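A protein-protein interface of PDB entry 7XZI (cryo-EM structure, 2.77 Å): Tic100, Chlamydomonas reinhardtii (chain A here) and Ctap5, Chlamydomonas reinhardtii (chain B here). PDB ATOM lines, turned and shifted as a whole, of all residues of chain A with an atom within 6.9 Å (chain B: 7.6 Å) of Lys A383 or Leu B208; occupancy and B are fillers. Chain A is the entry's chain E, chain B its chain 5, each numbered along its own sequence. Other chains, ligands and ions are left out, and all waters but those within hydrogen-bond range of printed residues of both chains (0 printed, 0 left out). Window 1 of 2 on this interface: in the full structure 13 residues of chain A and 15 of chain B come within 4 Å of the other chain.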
ATOM      1  N   GLU A 358      34.496 -33.036 -23.781  1.00  0.00           N
ATOM      2  CA  GLU A 358      34.357 -32.187 -24.958  1.00  0.00           C
ATOM      3  C   GLU A 358      32.915 -31.744 -25.164  1.00  0.00           C
ATOM      4  O   GLU A 358      32.670 -30.674 -25.731  1.00  0.00           O
ATOM      5  CB  GLU A 358      34.876 -32.923 -26.195  1.00  0.00           C
ATOM      6  CG  GLU A 358      34.841 -32.111 -27.478  1.00  0.00           C
ATOM      7  CD  GLU A 358      35.498 -32.832 -28.637  1.00  0.00           C
ATOM      8  OE1 GLU A 358      36.383 -33.677 -28.387  1.00  0.00           O
ATOM      9  OE2 GLU A 358      35.126 -32.560 -29.797  1.00  0.00           O
ATOM     10  N   ALA A 359      31.954 -32.544 -24.703  1.00  0.00           N
ATOM     11  CA  ALA A 359      30.547 -32.207 -24.890  1.00  0.00           C
ATOM     12  C   ALA A 359      30.111 -31.065 -23.981  1.00  0.00           C
ATOM     13  O   ALA A 359      29.392 -30.161 -24.420  1.00  0.00           O
ATOM     14  CB  ALA A 359      29.678 -33.441 -24.648  1.00  0.00           C
ATOM     15  N   SER A 360      30.533 -31.086 -22.718  1.00  0.00           N
ATOM     16  CA  SER A 360      30.103 -30.088 -21.746  1.00  0.00           C
ATOM     17  C   SER A 360      31.121 -28.980 -21.520  1.00  0.00           C
ATOM     18  O   SER A 360      30.731 -27.867 -21.153  1.00  0.00           O
ATOM     19  CB  SER A 360      29.786 -30.757 -20.404  1.00  0.00           C
ATOM     20  OG  SER A 360      30.933 -31.391 -19.867  1.00  0.00           O
ATOM     21  N   GLY A 361      32.408 -29.251 -21.723  1.00  0.00           N
ATOM     22  CA  GLY A 361      33.445 -28.257 -21.546  1.00  0.00           C
ATOM     23  C   GLY A 361      34.148 -28.296 -20.205  1.00  0.00           C
ATOM     24  O   GLY A 361      35.171 -27.620 -20.044  1.00  0.00           O
ATOM     25  N   GLU A 362      33.626 -29.051 -19.242  1.00  0.00           N
ATOM     26  CA  GLU A 362      34.255 -29.139 -17.933  1.00  0.00           C
ATOM     27  C   GLU A 362      35.643 -29.758 -18.039  1.00  0.00           C
ATOM     28  O   GLU A 362      35.836 -30.779 -18.702  1.00  0.00           O
ATOM     29  CB  GLU A 362      33.386 -29.968 -16.987  1.00  0.00           C
ATOM     30  CG  GLU A 362      34.035 -30.273 -15.644  1.00  0.00           C
ATOM     31  CD  GLU A 362      33.281 -31.330 -14.860  1.00  0.00           C
ATOM     32  OE1 GLU A 362      32.273 -31.851 -15.383  1.00  0.00           O
ATOM     33  OE2 GLU A 362      33.695 -31.643 -13.724  1.00  0.00           O
ATOM     34  N   LEU A 380      37.876 -25.829 -14.611  1.00  0.00           N
ATOM     35  CA  LEU A 380      37.659 -24.818 -15.632  1.00  0.00           C
ATOM     36  C   LEU A 380      36.439 -25.188 -16.465  1.00  0.00           C
ATOM     37  O   LEU A 380      36.098 -26.365 -16.612  1.00  0.00           O
ATOM     38  CB  LEU A 380      38.878 -24.668 -16.549  1.00  0.00           C
ATOM     39  CG  LEU A 380      40.221 -24.271 -15.934  1.00  0.00           C
ATOM     40  CD1 LEU A 380      40.960 -25.488 -15.402  1.00  0.00           C
ATOM     41  CD2 LEU A 380      41.075 -23.528 -16.949  1.00  0.00           C
ATOM     42  N   ASP A 381      35.784 -24.169 -17.013  1.00  0.00           N
ATOM     43  CA  ASP A 381      34.621 -24.346 -17.877  1.00  0.00           C
ATOM     44  C   ASP A 381      34.926 -23.667 -19.208  1.00  0.00           C
ATOM     45  O   ASP A 381      34.657 -22.478 -19.388  1.00  0.00           O
ATOM     46  CB  ASP A 381      33.364 -23.781 -17.231  1.00  0.00           C
ATOM     47  CG  ASP A 381      32.124 -24.016 -18.070  1.00  0.00           C
ATOM     48  OD1 ASP A 381      31.714 -25.188 -18.209  1.00  0.00           O
ATOM     49  OD2 ASP A 381      31.561 -23.031 -18.591  1.00  0.00           O
ATOM     50  N   MET A 382      35.492 -24.432 -20.142  1.00  0.00           N
ATOM     51  CA  MET A 382      35.846 -23.930 -21.461  1.00  0.00           C
ATOM     52  C   MET A 382      34.721 -24.105 -22.475  1.00  0.00           C
ATOM     53  O   MET A 382      34.993 -24.208 -23.677  1.00  0.00           O
ATOM     54  CB  MET A 382      37.119 -24.615 -21.963  1.00  0.00           C
ATOM     55  CG  MET A 382      38.303 -24.491 -21.021  1.00  0.00           C
ATOM     56  SD  MET A 382      39.855 -24.990 -21.791  1.00  0.00           S
ATOM     57  CE  MET A 382      40.057 -23.695 -23.012  1.00  0.00           C
ATOM     58  N   LYS A 383      33.470 -24.148 -22.017  1.00  0.00           N
ATOM     59  CA  LYS A 383      32.345 -24.342 -22.930  1.00  0.00           C
ATOM     60  C   LYS A 383      32.240 -23.264 -24.004  1.00  0.00           C
ATOM     61  O   LYS A 383      32.023 -23.621 -25.174  1.00  0.00           O
ATOM     62  CB  LYS A 383      31.045 -24.454 -22.129  1.00  0.00           C
ATOM     63  CG  LYS A 383      29.818 -24.701 -22.992  1.00  0.00           C
ATOM     64  CD  LYS A 383      30.019 -25.917 -23.881  1.00  0.00           C
ATOM     65  CE  LYS A 383      28.950 -26.011 -24.954  1.00  0.00           C
ATOM     66  NZ  LYS A 383      29.194 -27.163 -25.865  1.00  0.00           N
ATOM     67  N   PRO A 384      32.341 -21.962 -23.702  1.00  0.00           N
ATOM     68  CA  PRO A 384      32.237 -20.970 -24.787  1.00  0.00           C
ATOM     69  C   PRO A 384      33.313 -21.108 -25.849  1.00  0.00           C
ATOM     70  O   PRO A 384      33.036 -20.865 -27.032  1.00  0.00           O
ATOM     71  CB  PRO A 384      32.341 -19.627 -24.047  1.00  0.00           C
ATOM     72  CG  PRO A 384      33.017 -19.948 -22.769  1.00  0.00           C
ATOM     73  CD  PRO A 384      32.521 -21.305 -22.395  1.00  0.00           C
ATOM     74  N   TYR A 385      34.534 -21.494 -25.468  1.00  0.00           N
ATOM     75  CA  TYR A 385      35.594 -21.672 -26.457  1.00  0.00           C
ATOM     76  C   TYR A 385      35.244 -22.787 -27.435  1.00  0.00           C
ATOM     77  O   TYR A 385      35.371 -22.620 -28.652  1.00  0.00           O
ATOM     78  CB  TYR A 385      36.923 -21.961 -25.758  1.00  0.00           C
ATOM     79  CG  TYR A 385      38.069 -22.238 -26.704  1.00  0.00           C
ATOM     80  CD1 TYR A 385      38.581 -21.238 -27.518  1.00  0.00           C
ATOM     81  CD2 TYR A 385      38.648 -23.497 -26.775  1.00  0.00           C
ATOM     82  CE1 TYR A 385      39.629 -21.485 -28.382  1.00  0.00           C
ATOM     83  CE2 TYR A 385      39.698 -23.753 -27.635  1.00  0.00           C
ATOM     84  CZ  TYR A 385      40.185 -22.744 -28.436  1.00  0.00           C
ATOM     85  OH  TYR A 385      41.229 -22.990 -29.295  1.00  0.00           O
ATOM     86  N   PHE A 386      34.787 -23.929 -26.918  1.00  0.00           N
ATOM     87  CA  PHE A 386      34.372 -25.021 -27.792  1.00  0.00           C
ATOM     88  C   PHE A 386      33.155 -24.634 -28.619  1.00  0.00           C
ATOM     89  O   PHE A 386      33.039 -25.021 -29.787  1.00  0.00           O
ATOM     90  CB  PHE A 386      34.087 -26.274 -26.965  1.00  0.00           C
ATOM     91  CG  PHE A 386      35.298 -26.834 -26.277  1.00  0.00           C
ATOM     92  CD1 PHE A 386      36.571 -26.539 -26.735  1.00  0.00           C
ATOM     93  CD2 PHE A 386      35.164 -27.658 -25.173  1.00  0.00           C
ATOM     94  CE1 PHE A 386      37.685 -27.052 -26.104  1.00  0.00           C
ATOM     95  CE2 PHE A 386      36.274 -28.175 -24.539  1.00  0.00           C
ATOM     96  CZ  PHE A 386      37.536 -27.871 -25.005  1.00  0.00           C
ATOM     97  N   TYR A 387      32.231 -23.874 -28.027  1.00  0.00           N
ATOM     98  CA  TYR A 387      31.040 -23.440 -28.748  1.00  0.00           C
ATOM     99  C   TYR A 387      31.406 -22.576 -29.946  1.00  0.00           C
ATOM    100  O   TYR A 387      30.866 -22.760 -31.043  1.00  0.00           O
ATOM    101  CB  TYR A 387      30.109 -22.686 -27.796  1.00  0.00           C
ATOM    102  CG  TYR A 387      28.863 -22.124 -28.438  1.00  0.00           C
ATOM    103  CD1 TYR A 387      27.731 -22.909 -28.605  1.00  0.00           C
ATOM    104  CD2 TYR A 387      28.809 -20.803 -28.857  1.00  0.00           C
ATOM    105  CE1 TYR A 387      26.586 -22.397 -29.184  1.00  0.00           C
ATOM    106  CE2 TYR A 387      27.671 -20.282 -29.437  1.00  0.00           C
ATOM    107  CZ  TYR A 387      26.562 -21.083 -29.598  1.00  0.00           C
ATOM    108  OH  TYR A 387      25.426 -20.569 -30.175  1.00  0.00           O
ATOM    109  N   LEU A 388      32.324 -21.627 -29.758  1.00  0.00           N
ATOM    110  CA  LEU A 388      32.766 -20.803 -30.877  1.00  0.00           C
ATOM    111  C   LEU A 388      33.618 -21.595 -31.860  1.00  0.00           C
ATOM    112  O   LEU A 388      33.580 -21.327 -33.066  1.00  0.00           O
ATOM    113  CB  LEU A 388      33.535 -19.584 -30.370  1.00  0.00           C
ATOM    114  CG  LEU A 388      32.692 -18.447 -29.791  1.00  0.00           C
ATOM    115  CD1 LEU A 388      33.561 -17.245 -29.458  1.00  0.00           C
ATOM    116  CD2 LEU A 388      31.598 -18.067 -30.770  1.00  0.00           C
ATOM    117  N   LEU A 389      34.393 -22.566 -31.371  1.00  0.00           N
ATOM    118  CA  LEU A 389      35.225 -23.371 -32.260  1.00  0.00           C
ATOM    119  C   LEU A 389      34.372 -24.229 -33.185  1.00  0.00           C
ATOM    120  O   LEU A 389      34.703 -24.403 -34.364  1.00  0.00           O
ATOM    121  CB  LEU A 389      36.172 -24.241 -31.433  1.00  0.00           C
ATOM    122  CG  LEU A 389      37.534 -24.564 -32.046  1.00  0.00           C
ATOM    123  CD1 LEU A 389      38.259 -23.281 -32.399  1.00  0.00           C
ATOM    124  CD2 LEU A 389      38.360 -25.392 -31.081  1.00  0.00           C
ATOM    125  N   GLU A 390      33.271 -24.777 -32.669  1.00  0.00           N
ATOM    126  CA  GLU A 390      32.398 -25.637 -33.457  1.00  0.00           C
ATOM    127  C   GLU A 390      31.547 -24.876 -34.463  1.00  0.00           C
ATOM    128  O   GLU A 390      30.911 -25.511 -35.311  1.00  0.00           O
ATOM    129  CB  GLU A 390      31.482 -26.446 -32.535  1.00  0.00           C
ATOM    130  CG  GLU A 390      32.201 -27.459 -31.662  1.00  0.00           C
ATOM    131  CD  GLU A 390      31.295 -28.047 -30.597  1.00  0.00           C
ATOM    132  OE1 GLU A 390      30.176 -27.526 -30.413  1.00  0.00           O
ATOM    133  OE2 GLU A 390      31.701 -29.033 -29.946  1.00  0.00           O
ATOM    134  N   ARG A 391      31.513 -23.545 -34.398  1.00  0.00           N
ATOM    135  CA  ARG A 391      30.683 -22.741 -35.285  1.00  0.00           C
ATOM    136  C   ARG A 391      31.481 -22.086 -36.408  1.00  0.00           C
ATOM    137  O   ARG A 391      31.023 -21.098 -36.990  1.00  0.00           O
ATOM    138  CB  ARG A 391      29.927 -21.676 -34.487  1.00  0.00           C
ATOM    139  CG  ARG A 391      28.512 -22.078 -34.080  1.00  0.00           C
ATOM    140  CD  ARG A 391      28.513 -23.262 -33.127  1.00  0.00           C
ATOM    141  NE  ARG A 391      27.170 -23.627 -32.700  1.00  0.00           N
ATOM    142  CZ  ARG A 391      26.896 -24.577 -31.812  1.00  0.00           C
ATOM    143  NH1 ARG A 391      27.856 -25.276 -31.228  1.00  0.00           N
ATOM    144  NH2 ARG A 391      25.628 -24.828 -31.501  1.00  0.00           N
ATOM    145  N   ILE A 406      36.656 -17.122 -19.342  1.00  0.00           N
ATOM    146  CA  ILE A 406      37.110 -18.421 -18.859  1.00  0.00           C
ATOM    147  C   ILE A 406      38.144 -18.253 -17.751  1.00  0.00           C
ATOM    148  O   ILE A 406      38.127 -18.987 -16.755  1.00  0.00           O
ATOM    149  CB  ILE A 406      37.654 -19.265 -20.025  1.00  0.00           C
ATOM    150  CG1 ILE A 406      36.544 -19.542 -21.038  1.00  0.00           C
ATOM    151  CG2 ILE A 406      38.227 -20.574 -19.515  1.00  0.00           C
ATOM    152  CD1 ILE A 406      36.999 -20.346 -22.234  1.00  0.00           C
ATOM    153  N   ASP B 203      17.456 -36.180 -28.105  1.00  0.00           N
ATOM    154  CA  ASP B 203      17.707 -34.751 -28.276  1.00  0.00           C
ATOM    155  C   ASP B 203      17.325 -33.971 -27.025  1.00  0.00           C
ATOM    156  O   ASP B 203      18.015 -33.020 -26.641  1.00  0.00           O
ATOM    157  CB  ASP B 203      16.945 -34.222 -29.491  1.00  0.00           C
ATOM    158  CG  ASP B 203      17.466 -34.786 -30.798  1.00  0.00           C
ATOM    159  OD1 ASP B 203      18.417 -35.595 -30.760  1.00  0.00           O
ATOM    160  OD2 ASP B 203      16.927 -34.421 -31.863  1.00  0.00           O
ATOM    161  N   ARG B 204      16.221 -34.352 -26.380  1.00  0.00           N
ATOM    162  CA  ARG B 204      15.805 -33.674 -25.157  1.00  0.00           C
ATOM    163  C   ARG B 204      16.815 -33.880 -24.037  1.00  0.00           C
ATOM    164  O   ARG B 204      17.029 -32.974 -23.222  1.00  0.00           O
ATOM    165  CB  ARG B 204      14.419 -34.164 -24.731  1.00  0.00           C
ATOM    166  CG  ARG B 204      13.687 -33.240 -23.763  1.00  0.00           C
ATOM    167  CD  ARG B 204      13.967 -33.590 -22.308  1.00  0.00           C
ATOM    168  NE  ARG B 204      13.426 -34.891 -21.943  1.00  0.00           N
ATOM    169  CZ  ARG B 204      13.473 -35.406 -20.717  1.00  0.00           C
ATOM    170  NH1 ARG B 204      14.042 -34.755 -19.716  1.00  0.00           N
ATOM    171  NH2 ARG B 204      12.935 -36.600 -20.496  1.00  0.00           N
ATOM    172  N   LEU B 205      17.446 -35.054 -23.979  1.00  0.00           N
ATOM    173  CA  LEU B 205      18.439 -35.319 -22.947  1.00  0.00           C
ATOM    174  C   LEU B 205      19.757 -34.595 -23.187  1.00  0.00           C
ATOM    175  O   LEU B 205      20.508 -34.377 -22.231  1.00  0.00           O
ATOM    176  CB  LEU B 205      18.696 -36.824 -22.837  1.00  0.00           C
ATOM    177  CG  LEU B 205      17.543 -37.669 -22.294  1.00  0.00           C
ATOM    178  CD1 LEU B 205      17.909 -39.143 -22.295  1.00  0.00           C
ATOM    179  CD2 LEU B 205      17.168 -37.209 -20.896  1.00  0.00           C
ATOM    180  N   ASP B 206      20.051 -34.209 -24.427  1.00  0.00           N
ATOM    181  CA  ASP B 206      21.306 -33.531 -24.756  1.00  0.00           C
ATOM    182  C   ASP B 206      21.045 -32.551 -25.888  1.00  0.00           C
ATOM    183  O   ASP B 206      21.137 -32.902 -27.072  1.00  0.00           O
ATOM    184  CB  ASP B 206      22.402 -34.523 -25.139  1.00  0.00           C
ATOM    185  CG  ASP B 206      22.923 -35.310 -23.950  1.00  0.00           C
ATOM    186  OD1 ASP B 206      23.199 -34.692 -22.901  1.00  0.00           O
ATOM    187  OD2 ASP B 206      23.055 -36.547 -24.062  1.00  0.00           O
ATOM    188  N   PRO B 207      20.709 -31.300 -25.563  1.00  0.00           N
ATOM    189  CA  PRO B 207      20.338 -30.335 -26.609  1.00  0.00           C
ATOM    190  C   PRO B 207      21.523 -29.803 -27.402  1.00  0.00           C
ATOM    191  O   PRO B 207      21.399 -29.545 -28.605  1.00  0.00           O
ATOM    192  CB  PRO B 207      19.655 -29.206 -25.820  1.00  0.00           C
ATOM    193  CG  PRO B 207      19.392 -29.771 -24.448  1.00  0.00           C
ATOM    194  CD  PRO B 207      20.479 -30.761 -24.214  1.00  0.00           C
ATOM    195  N   LEU B 208      22.671 -29.625 -26.742  1.00  0.00           N
ATOM    196  CA  LEU B 208      23.810 -28.985 -27.395  1.00  0.00           C
ATOM    197  C   LEU B 208      24.389 -29.842 -28.515  1.00  0.00           C
ATOM    198  O   LEU B 208      24.806 -29.306 -29.547  1.00  0.00           O
ATOM    199  CB  LEU B 208      24.887 -28.655 -26.362  1.00  0.00           C
ATOM    200  CG  LEU B 208      24.507 -27.558 -25.364  1.00  0.00           C
ATOM    201  CD1 LEU B 208      25.622 -27.321 -24.358  1.00  0.00           C
ATOM    202  CD2 LEU B 208      24.160 -26.271 -26.098  1.00  0.00           C
ATOM    203  N   GLU B 209      24.433 -31.164 -28.332  1.00  0.00           N
ATOM    204  CA  GLU B 209      24.895 -32.036 -29.407  1.00  0.00           C
ATOM    205  C   GLU B 209      23.966 -31.959 -30.612  1.00  0.00           C
ATOM    206  O   GLU B 209      24.424 -31.929 -31.763  1.00  0.00           O
ATOM    207  CB  GLU B 209      25.008 -33.473 -28.903  1.00  0.00           C
ATOM    208  CG  GLU B 209      26.030 -33.652 -27.797  1.00  0.00           C
ATOM    209  CD  GLU B 209      27.439 -33.343 -28.256  1.00  0.00           C
ATOM    210  OE1 GLU B 209      27.769 -33.656 -29.420  1.00  0.00           O
ATOM    211  OE2 GLU B 209      28.216 -32.781 -27.458  1.00  0.00           O
ATOM    212  N   ALA B 210      22.655 -31.925 -30.365  1.00  0.00           N
ATOM    213  CA  ALA B 210      21.699 -31.771 -31.454  1.00  0.00           C
ATOM    214  C   ALA B 210      21.888 -30.437 -32.164  1.00  0.00           C
ATOM    215  O   ALA B 210      21.806 -30.364 -33.393  1.00  0.00           O
ATOM    216  CB  ALA B 210      20.273 -31.902 -30.924  1.00  0.00           C
ATOM    217  N   ASP B 211      22.141 -29.369 -31.403  1.00  0.00           N
ATOM    218  CA  ASP B 211      22.378 -28.065 -32.015  1.00  0.00           C
ATOM    219  C   ASP B 211      23.636 -28.080 -32.875  1.00  0.00           C
ATOM    220  O   ASP B 211      23.656 -27.509 -33.973  1.00  0.00           O
ATOM    221  CB  ASP B 211      22.480 -26.990 -30.933  1.00  0.00           C
ATOM    222  CG  ASP B 211      22.297 -25.590 -31.481  1.00  0.00           C
ATOM    223  OD1 ASP B 211      21.135 -25.185 -31.696  1.00  0.00           O
ATOM    224  OD2 ASP B 211      23.310 -24.894 -31.703  1.00  0.00           O
ATOM    225  N   ARG B 212      24.698 -28.724 -32.388  1.00  0.00           N
ATOM    226  CA  ARG B 212      25.935 -28.818 -33.159  1.00  0.00           C
ATOM    227  C   ARG B 212      25.718 -29.592 -34.454  1.00  0.00           C
ATOM    228  O   ARG B 212      26.189 -29.184 -35.522  1.00  0.00           O
ATOM    229  CB  ARG B 212      27.025 -29.477 -32.315  1.00  0.00           C
ATOM    230  CG  ARG B 212      28.344 -29.675 -33.042  1.00  0.00           C
ATOM    231  CD  ARG B 212      29.348 -30.400 -32.164  1.00  0.00           C
ATOM    232  NE  ARG B 212      28.943 -31.770 -31.884  1.00  0.00           N
ATOM    233  CZ  ARG B 212      29.339 -32.826 -32.587  1.00  0.00           C
ATOM    234  NH1 ARG B 212      30.162 -32.703 -33.615  1.00  0.00           N
ATOM    235  NH2 ARG B 212      28.898 -34.033 -32.247  1.00  0.00           N
ATOM    236  N   ARG B 213      25.002 -30.716 -34.376  1.00  0.00           N
ATOM    237  CA  ARG B 213      24.738 -31.497 -35.582  1.00  0.00           C
ATOM    238  C   ARG B 213      23.840 -30.733 -36.548  1.00  0.00           C
ATOM    239  O   ARG B 213      24.010 -30.829 -37.770  1.00  0.00           O
ATOM    240  CB  ARG B 213      24.121 -32.845 -35.215  1.00  0.00           C
ATOM    241  CG  ARG B 213      25.070 -33.770 -34.467  1.00  0.00           C
ATOM    242  CD  ARG B 213      24.508 -35.177 -34.357  1.00  0.00           C
ATOM    243  NE  ARG B 213      25.460 -36.095 -33.747  1.00  0.00           N
ATOM    244  CZ  ARG B 213      25.491 -36.394 -32.453  1.00  0.00           C
ATOM    245  NH1 ARG B 213      24.625 -35.870 -31.601  1.00  0.00           N
ATOM    246  NH2 ARG B 213      26.414 -37.240 -32.004  1.00  0.00           N
ATOM    247  N   ALA B 214      22.883 -29.966 -36.023  1.00  0.00           N
ATOM    248  CA  ALA B 214      22.045 -29.135 -36.880  1.00  0.00           C
ATOM    249  C   ALA B 214      22.870 -28.070 -37.591  1.00  0.00           C
ATOM    250  O   ALA B 214      22.665 -27.809 -38.781  1.00  0.00           O
ATOM    251  CB  ALA B 214      20.928 -28.492 -36.060  1.00  0.00           C
ATOM    252  N   TYR B 227      19.617 -21.389 -40.023  1.00  0.00           N
ATOM    253  CA  TYR B 227      20.051 -21.897 -38.725  1.00  0.00           C
ATOM    254  C   TYR B 227      20.032 -20.793 -37.675  1.00  0.00           C
ATOM    255  O   TYR B 227      19.435 -20.949 -36.604  1.00  0.00           O
ATOM    256  CB  TYR B 227      21.449 -22.505 -38.838  1.00  0.00           C
ATOM    257  CG  TYR B 227      22.084 -22.840 -37.504  1.00  0.00           C
ATOM    258  CD1 TYR B 227      21.824 -24.049 -36.874  1.00  0.00           C
ATOM    259  CD2 TYR B 227      22.946 -21.950 -36.879  1.00  0.00           C
ATOM    260  CE1 TYR B 227      22.401 -24.358 -35.657  1.00  0.00           C
ATOM    261  CE2 TYR B 227      23.524 -22.250 -35.662  1.00  0.00           C
ATOM    262  CZ  TYR B 227      23.251 -23.456 -35.057  1.00  0.00           C
ATOM    263  OH  TYR B 227      23.828 -23.758 -33.847  1.00  0.00           O
ATOM    264  N   THR B 236      20.985 -18.133 -27.143  1.00  0.00           N
ATOM    265  CA  THR B 236      21.998 -19.009 -26.563  1.00  0.00           C
ATOM    266  C   THR B 236      23.406 -18.515 -26.872  1.00  0.00           C
ATOM    267  O   THR B 236      24.307 -18.671 -26.042  1.00  0.00           O
ATOM    268  CB  THR B 236      21.805 -20.450 -27.044  1.00  0.00           C
ATOM    269  OG1 THR B 236      22.780 -21.297 -26.420  1.00  0.00           O
ATOM    270  CG2 THR B 236      21.946 -20.553 -28.551  1.00  0.00           C
ATOM    271  N   ARG B 239      23.972 -15.867 -24.342  1.00  0.00           N
ATOM    272  CA  ARG B 239      24.157 -16.433 -23.011  1.00  0.00           C
ATOM    273  C   ARG B 239      25.538 -17.060 -22.853  1.00  0.00           C
ATOM    274  O   ARG B 239      26.185 -16.893 -21.813  1.00  0.00           O
ATOM    275  CB  ARG B 239      23.065 -17.462 -22.725  1.00  0.00           C
ATOM    276  CG  ARG B 239      23.179 -18.127 -21.365  1.00  0.00           C
ATOM    277  CD  ARG B 239      22.034 -19.094 -21.126  1.00  0.00           C
ATOM    278  NE  ARG B 239      21.989 -20.143 -22.135  1.00  0.00           N
ATOM    279  CZ  ARG B 239      22.614 -21.311 -22.031  1.00  0.00           C
ATOM    280  NH1 ARG B 239      23.340 -21.614 -20.968  1.00  0.00           N
ATOM    281  NH2 ARG B 239      22.507 -22.195 -23.019  1.00  0.00           N
ATOM    282  N   ILE B 240      26.006 -17.784 -23.869  1.00  0.00           N
ATOM    283  CA  ILE B 240      27.257 -18.525 -23.741  1.00  0.00           C
ATOM    284  C   ILE B 240      28.455 -17.616 -23.981  1.00  0.00           C
ATOM    285  O   ILE B 240      29.346 -17.506 -23.130  1.00  0.00           O
ATOM    286  CB  ILE B 240      27.258 -19.731 -24.698  1.00  0.00           C
ATOM    287  CG1 ILE B 240      26.141 -20.707 -24.327  1.00  0.00           C
ATOM    288  CG2 ILE B 240      28.601 -20.431 -24.671  1.00  0.00           C
ATOM    289  CD1 ILE B 240      26.045 -21.905 -25.244  1.00  0.00           C
ATOM    290  N   VAL B 241      28.502 -16.955 -25.140  1.00  0.00           N
ATOM    291  CA  VAL B 241      29.651 -16.118 -25.472  1.00  0.00           C
ATOM    292  C   VAL B 241      29.717 -14.904 -24.556  1.00  0.00           C
ATOM    293  O   VAL B 241      30.792 -14.535 -24.066  1.00  0.00           O
ATOM    294  CB  VAL B 241      29.594 -15.705 -26.954  1.00  0.00           C
ATOM    295  CG1 VAL B 241      30.802 -14.854 -27.315  1.00  0.00           C
ATOM    296  CG2 VAL B 241      29.513 -16.934 -27.844  1.00  0.00           C
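OH of Tyr B227 sits at hydrogen-bond distance from NH2 of Arg A391, 3.1 Å away. OD2 of Asp B211 lies close to NH2 of Arg A391, 2.3 Å away.
O of Ala A359 sits at hydrogen-bond distance from NZ of Lys A383, 3.3 Å away. OE1 of Glu B209 lies within salt-bridge range of NH2 of Arg B212. The side-chain carboxylate of Asp B211 lies within hydrogen-bond range of the side-chain hydroxyl of Tyr B227, at 2.5 Å. The side-chain carboxylate of Glu A390 lies within salt-bridge range of the guanidinium group of Arg A391, 3.3 Å away.
Glu B209 touches Ala A359. Lys A383 touches Leu B208. CG2 of Ile B240 touches CA of Pro A384, 3.7 Å away. Tyr A387 touches Thr B236. CD1 of Ile B240 touches CD1 of Tyr A387, at 3.9 Å. Leu A388 touches Val B241 (CD2 to CG2, 3.8 Å). Arg B212 touches Glu A390 (CD to CD, 3.4 Å).
Leu B208 touches just one residue of chain A: Lys A383 (3.6 Å). Of the printed residues of chain B, Tyr A387 touches Thr B236 and Ile B240. Of the printed residues of chain B, Pro A384 touches Ile B240 (3.7 Å). Of the printed residues of chain A, Asp B211 touches Arg A391 (2.3 Å). Printed residues of chain A within 4 Å of Ile B240: Pro A384 (3.7 Å) and Tyr A387 (3.9 Å). The nearest residue of chain B that does not touch Lys A383 is Ile B240 (4.7 Å). The nearest printed residue of chain B that does not touch Glu A390 is Glu B209 (5.7 Å).
Of the 17 printed residues of chain B, 8 touch a printed residue of chain A. Hydrophobic or aromatic side chains of chain B that line the printed part of chain A: Leu B208, Tyr B227, Ile B240 and Val B241. Of the 18 printed residues of chain A, 7 touch a printed residue of chain B. Hydrophobic or aromatic side chains of chain A that line the printed part of chain B: Ala A359, Pro A384, Tyr A387 and Leu A388. Among the printed residues, 9 pairs touch across the chains. Among the printed residues, Asp or Glu carboxylates within 4 Å of a Lys or Arg side-chain nitrogen of the other chain: Arg A391 with Asp B211 (2.3 Å).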
